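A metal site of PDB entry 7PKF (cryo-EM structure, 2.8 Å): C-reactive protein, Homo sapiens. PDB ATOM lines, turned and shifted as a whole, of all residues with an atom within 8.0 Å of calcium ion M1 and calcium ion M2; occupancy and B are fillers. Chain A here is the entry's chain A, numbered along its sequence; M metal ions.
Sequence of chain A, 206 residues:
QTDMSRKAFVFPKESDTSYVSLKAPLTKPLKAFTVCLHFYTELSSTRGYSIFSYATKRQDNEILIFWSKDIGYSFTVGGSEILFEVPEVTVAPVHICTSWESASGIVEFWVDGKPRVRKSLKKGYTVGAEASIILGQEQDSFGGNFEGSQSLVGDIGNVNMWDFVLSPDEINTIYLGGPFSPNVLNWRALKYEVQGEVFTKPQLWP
NE2 of Gln 139 lies within hydrogen-bond range of OG of Ser 53 (3.0 Å). The side-chain amide oxygen (OD1) of Asn 61 lies close to the side-chain carboxylate (OD1) of Asp 60. The side-chain amide oxygen of Gln 59 lies within hydrogen-bond range of the backbone NH of Asn 61 (2.9 Å). The backbone NH (N) of Ser 50 is in hydrogen-bond range of the backbone carbonyl oxygen (O) of Gln 150, at 2.9 Å. The side-chain carboxylate (OD1) of Asp 60 sits close to the side-chain amide oxygen (OE1) of Gln 59.
Merely in contact with calcium ion M1: Asp 60. The nearest printed residue that does not touch calcium ion M1 is Leu 64 (5.3 Å).
Four residues have an atom within 4 Å of calcium ion M2: Glu 138, Asp 140, Glu 147 and Gln 150.
Calcium ion M1 is bound by the side-chain carboxylate (OE2) of Glu 138 (2.3 Å), the backbone carbonyl oxygen (O) of Gln 139 (2.3 Å), the side-chain carboxylate (OD2) of Asp 140 (2.5 Å), the side-chain amide oxygen (OD1) of Asn 61 (2.5 Å) and the side-chain carboxylate (OE1) of Glu 138 (2.8 Å).
Calcium ion M2 is bound by OE1 of Glu 138 (2.4 Å). Calcium ion M2 is bound by OD1 of Asp 140 (2.4 Å). OE1 of Gln 150 is bound to calcium ion M2, at 2.6 Å. OD2 of Asp 140 binds calcium ion M2, 2.6 Å away. Calcium ion M2 has four donor atoms within binding distance. Slightly farther from calcium ion M2 lies OE1 of Glu 147 (2.9 Å).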
ATOM      1  N   SER A  50      19.316  -4.175 -20.146  1.00  0.00           N
ATOM      2  CA  SER A  50      18.376  -5.272 -20.352  1.00  0.00           C
ATOM      3  C   SER A  50      17.182  -4.846 -21.209  1.00  0.00           C
ATOM      4  O   SER A  50      16.493  -3.875 -20.891  1.00  0.00           O
ATOM      5  CB  SER A  50      17.896  -5.802 -19.012  1.00  0.00           C
ATOM      6  OG  SER A  50      16.932  -6.828 -19.180  1.00  0.00           O
ATOM      7  N   SER A  53      14.044  -9.686 -19.783  1.00  0.00           N
ATOM      8  CA  SER A  53      14.587 -10.542 -18.733  1.00  0.00           C
ATOM      9  C   SER A  53      13.548 -11.571 -18.305  1.00  0.00           C
ATOM     10  O   SER A  53      12.468 -11.217 -17.837  1.00  0.00           O
ATOM     11  CB  SER A  53      15.020  -9.705 -17.527  1.00  0.00           C
ATOM     12  OG  SER A  53      15.550 -10.536 -16.502  1.00  0.00           O
ATOM     13  N   TYR A  54      13.880 -12.849 -18.497  1.00  0.00           N
ATOM     14  CA  TYR A  54      13.069 -13.975 -18.060  1.00  0.00           C
ATOM     15  C   TYR A  54      13.893 -14.788 -17.078  1.00  0.00           C
ATOM     16  O   TYR A  54      14.957 -15.302 -17.428  1.00  0.00           O
ATOM     17  CB  TYR A  54      12.689 -14.803 -19.293  1.00  0.00           C
ATOM     18  CG  TYR A  54      11.796 -16.005 -19.144  1.00  0.00           C
ATOM     19  CD1 TYR A  54      12.205 -17.125 -18.448  1.00  0.00           C
ATOM     20  CD2 TYR A  54      10.556 -16.044 -19.777  1.00  0.00           C
ATOM     21  CE1 TYR A  54      11.387 -18.232 -18.346  1.00  0.00           C
ATOM     22  CE2 TYR A  54       9.744 -17.142 -19.684  1.00  0.00           C
ATOM     23  CZ  TYR A  54      10.173 -18.240 -18.977  1.00  0.00           C
ATOM     24  OH  TYR A  54       9.362 -19.352 -18.887  1.00  0.00           O
ATOM     25  N   ALA A  55      13.388 -14.916 -15.849  1.00  0.00           N
ATOM     26  CA  ALA A  55      14.088 -15.605 -14.775  1.00  0.00           C
ATOM     27  C   ALA A  55      13.233 -16.727 -14.186  1.00  0.00           C
ATOM     28  O   ALA A  55      12.009 -16.590 -14.092  1.00  0.00           O
ATOM     29  CB  ALA A  55      14.473 -14.634 -13.651  1.00  0.00           C
ATOM     30  N   GLN A  59      17.386 -20.024 -12.127  1.00  0.00           N
ATOM     31  CA  GLN A  59      18.256 -19.428 -13.138  1.00  0.00           C
ATOM     32  C   GLN A  59      17.740 -18.028 -13.451  1.00  0.00           C
ATOM     33  O   GLN A  59      16.655 -17.874 -14.002  1.00  0.00           O
ATOM     34  CB  GLN A  59      18.294 -20.288 -14.391  1.00  0.00           C
ATOM     35  CG  GLN A  59      19.088 -19.701 -15.545  1.00  0.00           C
ATOM     36  CD  GLN A  59      20.485 -19.302 -15.143  1.00  0.00           C
ATOM     37  OE1 GLN A  59      20.771 -18.120 -14.922  1.00  0.00           O
ATOM     38  NE2 GLN A  59      21.372 -20.286 -15.032  1.00  0.00           N
ATOM     39  N   ASP A  60      18.531 -17.009 -13.091  1.00  0.00           N
ATOM     40  CA  ASP A  60      18.113 -15.619 -13.267  1.00  0.00           C
ATOM     41  C   ASP A  60      18.219 -15.152 -14.713  1.00  0.00           C
ATOM     42  O   ASP A  60      17.577 -14.165 -15.078  1.00  0.00           O
ATOM     43  CB  ASP A  60      18.953 -14.702 -12.379  1.00  0.00           C
ATOM     44  CG  ASP A  60      20.424 -14.707 -12.756  1.00  0.00           C
ATOM     45  OD1 ASP A  60      20.806 -15.464 -13.667  1.00  0.00           O
ATOM     46  OD2 ASP A  60      21.204 -13.963 -12.124  1.00  0.00           O
ATOM     47  N   ASN A  61      19.016 -15.840 -15.533  1.00  0.00           N
ATOM     48  CA  ASN A  61      19.156 -15.507 -16.946  1.00  0.00           C
ATOM     49  C   ASN A  61      18.617 -16.634 -17.806  1.00  0.00           C
ATOM     50  O   ASN A  61      19.319 -17.137 -18.692  1.00  0.00           O
ATOM     51  CB  ASN A  61      20.621 -15.236 -17.295  1.00  0.00           C
ATOM     52  CG  ASN A  61      21.153 -13.989 -16.650  1.00  0.00           C
ATOM     53  OD1 ASN A  61      20.403 -13.199 -16.087  1.00  0.00           O
ATOM     54  ND2 ASN A  61      22.463 -13.796 -16.732  1.00  0.00           N
ATOM     55  N   GLU A  62      17.370 -17.055 -17.558  1.00  0.00           N
ATOM     56  CA  GLU A  62      16.843 -18.198 -18.289  1.00  0.00           C
ATOM     57  C   GLU A  62      16.509 -17.835 -19.734  1.00  0.00           C
ATOM     58  O   GLU A  62      16.791 -18.613 -20.653  1.00  0.00           O
ATOM     59  CB  GLU A  62      15.603 -18.723 -17.557  1.00  0.00           C
ATOM     60  CG  GLU A  62      14.911 -19.902 -18.216  1.00  0.00           C
ATOM     61  CD  GLU A  62      15.603 -21.200 -17.903  1.00  0.00           C
ATOM     62  OE1 GLU A  62      14.911 -22.240 -17.830  1.00  0.00           O
ATOM     63  OE2 GLU A  62      16.832 -21.197 -17.738  1.00  0.00           O
ATOM     64  N   LEU A  64      17.474 -14.003 -21.484  1.00  0.00           N
ATOM     65  CA  LEU A  64      17.781 -12.587 -21.390  1.00  0.00           C
ATOM     66  C   LEU A  64      18.209 -12.078 -22.756  1.00  0.00           C
ATOM     67  O   LEU A  64      19.089 -12.648 -23.395  1.00  0.00           O
ATOM     68  CB  LEU A  64      18.858 -12.314 -20.342  1.00  0.00           C
ATOM     69  CG  LEU A  64      19.447 -10.895 -20.282  1.00  0.00           C
ATOM     70  CD1 LEU A  64      18.464  -9.928 -19.651  1.00  0.00           C
ATOM     71  CD2 LEU A  64      20.753 -10.903 -19.525  1.00  0.00           C
ATOM     72  N   PHE A  66      19.932  -8.744 -24.157  1.00  0.00           N
ATOM     73  CA  PHE A  66      20.743  -7.687 -23.568  1.00  0.00           C
ATOM     74  C   PHE A  66      21.493  -6.962 -24.671  1.00  0.00           C
ATOM     75  O   PHE A  66      22.011  -7.597 -25.592  1.00  0.00           O
ATOM     76  CB  PHE A  66      21.720  -8.278 -22.541  1.00  0.00           C
ATOM     77  CG  PHE A  66      22.209  -7.284 -21.532  1.00  0.00           C
ATOM     78  CD1 PHE A  66      21.533  -7.088 -20.344  1.00  0.00           C
ATOM     79  CD2 PHE A  66      23.386  -6.586 -21.752  1.00  0.00           C
ATOM     80  CE1 PHE A  66      22.002  -6.191 -19.400  1.00  0.00           C
ATOM     81  CE2 PHE A  66      23.853  -5.687 -20.818  1.00  0.00           C
ATOM     82  CZ  PHE A  66      23.162  -5.491 -19.637  1.00  0.00           C
ATOM     83  N   THR A  76      20.894 -14.845 -24.481  1.00  0.00           N
ATOM     84  CA  THR A  76      21.301 -15.956 -23.639  1.00  0.00           C
ATOM     85  C   THR A  76      20.090 -16.742 -23.162  1.00  0.00           C
ATOM     86  O   THR A  76      19.055 -16.161 -22.806  1.00  0.00           O
ATOM     87  CB  THR A  76      22.119 -15.476 -22.432  1.00  0.00           C
ATOM     88  OG1 THR A  76      22.512 -16.600 -21.641  1.00  0.00           O
ATOM     89  CG2 THR A  76      21.317 -14.512 -21.584  1.00  0.00           C
ATOM     90  N   GLN A 137      14.285  -3.883 -16.260  1.00  0.00           N
ATOM     91  CA  GLN A 137      15.356  -4.223 -15.337  1.00  0.00           C
ATOM     92  C   GLN A 137      15.933  -5.565 -15.733  1.00  0.00           C
ATOM     93  O   GLN A 137      15.308  -6.341 -16.467  1.00  0.00           O
ATOM     94  CB  GLN A 137      14.864  -4.254 -13.889  1.00  0.00           C
ATOM     95  CG  GLN A 137      14.313  -2.939 -13.379  1.00  0.00           C
ATOM     96  CD  GLN A 137      15.364  -1.849 -13.315  1.00  0.00           C
ATOM     97  OE1 GLN A 137      16.560  -2.128 -13.204  1.00  0.00           O
ATOM     98  NE2 GLN A 137      14.928  -0.592 -13.368  1.00  0.00           N
ATOM     99  N   GLU A 138      17.129  -5.860 -15.223  1.00  0.00           N
ATOM    100  CA  GLU A 138      17.774  -7.151 -15.395  1.00  0.00           C
ATOM    101  C   GLU A 138      17.760  -7.871 -14.059  1.00  0.00           C
ATOM    102  O   GLU A 138      18.317  -7.388 -13.067  1.00  0.00           O
ATOM    103  CB  GLU A 138      19.209  -6.979 -15.890  1.00  0.00           C
ATOM    104  CG  GLU A 138      19.779  -8.199 -16.592  1.00  0.00           C
ATOM    105  CD  GLU A 138      20.477  -9.153 -15.645  1.00  0.00           C
ATOM    106  OE1 GLU A 138      20.620  -8.815 -14.448  1.00  0.00           O
ATOM    107  OE2 GLU A 138      20.889 -10.239 -16.093  1.00  0.00           O
ATOM    108  N   GLN A 139      17.120  -9.044 -14.027  1.00  0.00           N
ATOM    109  CA  GLN A 139      17.026  -9.810 -12.789  1.00  0.00           C
ATOM    110  C   GLN A 139      18.332 -10.525 -12.493  1.00  0.00           C
ATOM    111  O   GLN A 139      18.963 -11.100 -13.380  1.00  0.00           O
ATOM    112  CB  GLN A 139      15.889 -10.826 -12.898  1.00  0.00           C
ATOM    113  CG  GLN A 139      14.511 -10.209 -12.860  1.00  0.00           C
ATOM    114  CD  GLN A 139      13.430 -11.166 -13.296  1.00  0.00           C
ATOM    115  OE1 GLN A 139      12.651 -11.660 -12.478  1.00  0.00           O
ATOM    116  NE2 GLN A 139      13.375 -11.442 -14.589  1.00  0.00           N
ATOM    117  N   ASP A 140      18.727 -10.490 -11.224  1.00  0.00           N
ATOM    118  CA  ASP A 140      19.754 -11.373 -10.697  1.00  0.00           C
ATOM    119  C   ASP A 140      19.216 -12.323  -9.646  1.00  0.00           C
ATOM    120  O   ASP A 140      19.954 -13.212  -9.188  1.00  0.00           O
ATOM    121  CB  ASP A 140      20.917 -10.568 -10.105  1.00  0.00           C
ATOM    122  CG  ASP A 140      21.697  -9.805 -11.164  1.00  0.00           C
ATOM    123  OD1 ASP A 140      22.100  -8.656 -10.906  1.00  0.00           O
ATOM    124  OD2 ASP A 140      21.900 -10.354 -12.267  1.00  0.00           O
ATOM    125  N   SER A 141      17.954 -12.168  -9.245  1.00  0.00           N
ATOM    126  CA  SER A 141      17.217 -13.161  -8.479  1.00  0.00           C
ATOM    127  C   SER A 141      15.781 -13.148  -8.979  1.00  0.00           C
ATOM    128  O   SER A 141      15.362 -12.239  -9.710  1.00  0.00           O
ATOM    129  CB  SER A 141      17.270 -12.866  -6.978  1.00  0.00           C
ATOM    130  OG  SER A 141      16.512 -11.722  -6.650  1.00  0.00           O
ATOM    131  N   GLY A 144      13.884  -9.804  -8.665  1.00  0.00           N
ATOM    132  CA  GLY A 144      14.557  -8.798  -7.868  1.00  0.00           C
ATOM    133  C   GLY A 144      16.041  -8.727  -8.142  1.00  0.00           C
ATOM    134  O   GLY A 144      16.546  -9.258  -9.125  1.00  0.00           O
ATOM    135  N   ASN A 145      16.738  -8.043  -7.230  1.00  0.00           N
ATOM    136  CA  ASN A 145      18.159  -7.732  -7.349  1.00  0.00           C
ATOM    137  C   ASN A 145      18.472  -7.027  -8.663  1.00  0.00           C
ATOM    138  O   ASN A 145      19.321  -7.448  -9.456  1.00  0.00           O
ATOM    139  CB  ASN A 145      18.997  -9.002  -7.198  1.00  0.00           C
ATOM    140  CG  ASN A 145      18.974  -9.548  -5.790  1.00  0.00           C
ATOM    141  OD1 ASN A 145      18.222 -10.472  -5.481  1.00  0.00           O
ATOM    142  ND2 ASN A 145      19.792  -8.977  -4.916  1.00  0.00           N
ATOM    143  N   PHE A 146      17.768  -5.916  -8.904  1.00  0.00           N
ATOM    144  CA  PHE A 146      17.987  -5.112 -10.094  1.00  0.00           C
ATOM    145  C   PHE A 146      19.262  -4.289  -9.969  1.00  0.00           C
ATOM    146  O   PHE A 146      19.717  -3.972  -8.866  1.00  0.00           O
ATOM    147  CB  PHE A 146      16.781  -4.210 -10.343  1.00  0.00           C
ATOM    148  CG  PHE A 146      15.470  -4.931 -10.332  1.00  0.00           C
ATOM    149  CD1 PHE A 146      15.283  -6.054 -11.134  1.00  0.00           C
ATOM    150  CD2 PHE A 146      14.437  -4.514  -9.521  1.00  0.00           C
ATOM    151  CE1 PHE A 146      14.089  -6.729 -11.123  1.00  0.00           C
ATOM    152  CE2 PHE A 146      13.227  -5.189  -9.519  1.00  0.00           C
ATOM    153  CZ  PHE A 146      13.061  -6.303 -10.322  1.00  0.00           C
ATOM    154  N   GLU A 147      19.831  -3.932 -11.116  1.00  0.00           N
ATOM    155  CA  GLU A 147      20.953  -3.000 -11.184  1.00  0.00           C
ATOM    156  C   GLU A 147      20.562  -1.810 -12.056  1.00  0.00           C
ATOM    157  O   GLU A 147      20.176  -1.987 -13.217  1.00  0.00           O
ATOM    158  CB  GLU A 147      22.192  -3.687 -11.766  1.00  0.00           C
ATOM    159  CG  GLU A 147      22.815  -4.733 -10.864  1.00  0.00           C
ATOM    160  CD  GLU A 147      23.968  -5.450 -11.520  1.00  0.00           C
ATOM    161  OE1 GLU A 147      24.179  -6.648 -11.227  1.00  0.00           O
ATOM    162  OE2 GLU A 147      24.675  -4.818 -12.334  1.00  0.00           O
ATOM    163  N   GLY A 148      20.665  -0.608 -11.484  1.00  0.00           N
ATOM    164  CA  GLY A 148      20.299   0.594 -12.215  1.00  0.00           C
ATOM    165  C   GLY A 148      21.151   0.826 -13.450  1.00  0.00           C
ATOM    166  O   GLY A 148      20.665   1.347 -14.454  1.00  0.00           O
ATOM    167  N   SER A 149      22.429   0.467 -13.375  1.00  0.00           N
ATOM    168  CA  SER A 149      23.323   0.543 -14.530  1.00  0.00           C
ATOM    169  C   SER A 149      22.921  -0.400 -15.657  1.00  0.00           C
ATOM    170  O   SER A 149      23.455  -0.263 -16.765  1.00  0.00           O
ATOM    171  CB  SER A 149      24.748   0.230 -14.091  1.00  0.00           C
ATOM    172  OG  SER A 149      24.842  -1.065 -13.529  1.00  0.00           O
ATOM    173  N   GLN A 150      22.019  -1.340 -15.410  1.00  0.00           N
ATOM    174  CA  GLN A 150      21.493  -2.224 -16.445  1.00  0.00           C
ATOM    175  C   GLN A 150      20.049  -1.936 -16.835  1.00  0.00           C
ATOM    176  O   GLN A 150      19.528  -2.610 -17.721  1.00  0.00           O
ATOM    177  CB  GLN A 150      21.628  -3.678 -15.979  1.00  0.00           C
ATOM    178  CG  GLN A 150      23.060  -4.106 -15.735  1.00  0.00           C
ATOM    179  CD  GLN A 150      23.227  -5.608 -15.692  1.00  0.00           C
ATOM    180  OE1 GLN A 150      22.410  -6.321 -15.112  1.00  0.00           O
ATOM    181  NE2 GLN A 150      24.296  -6.102 -16.307  1.00  0.00           N
HETATM  182 CA    CA M   1      21.047 -11.576 -14.275  1.00  0.00          CA
HETATM  183 CA    CA M   2      22.386  -7.954 -13.141  1.00  0.00          CA
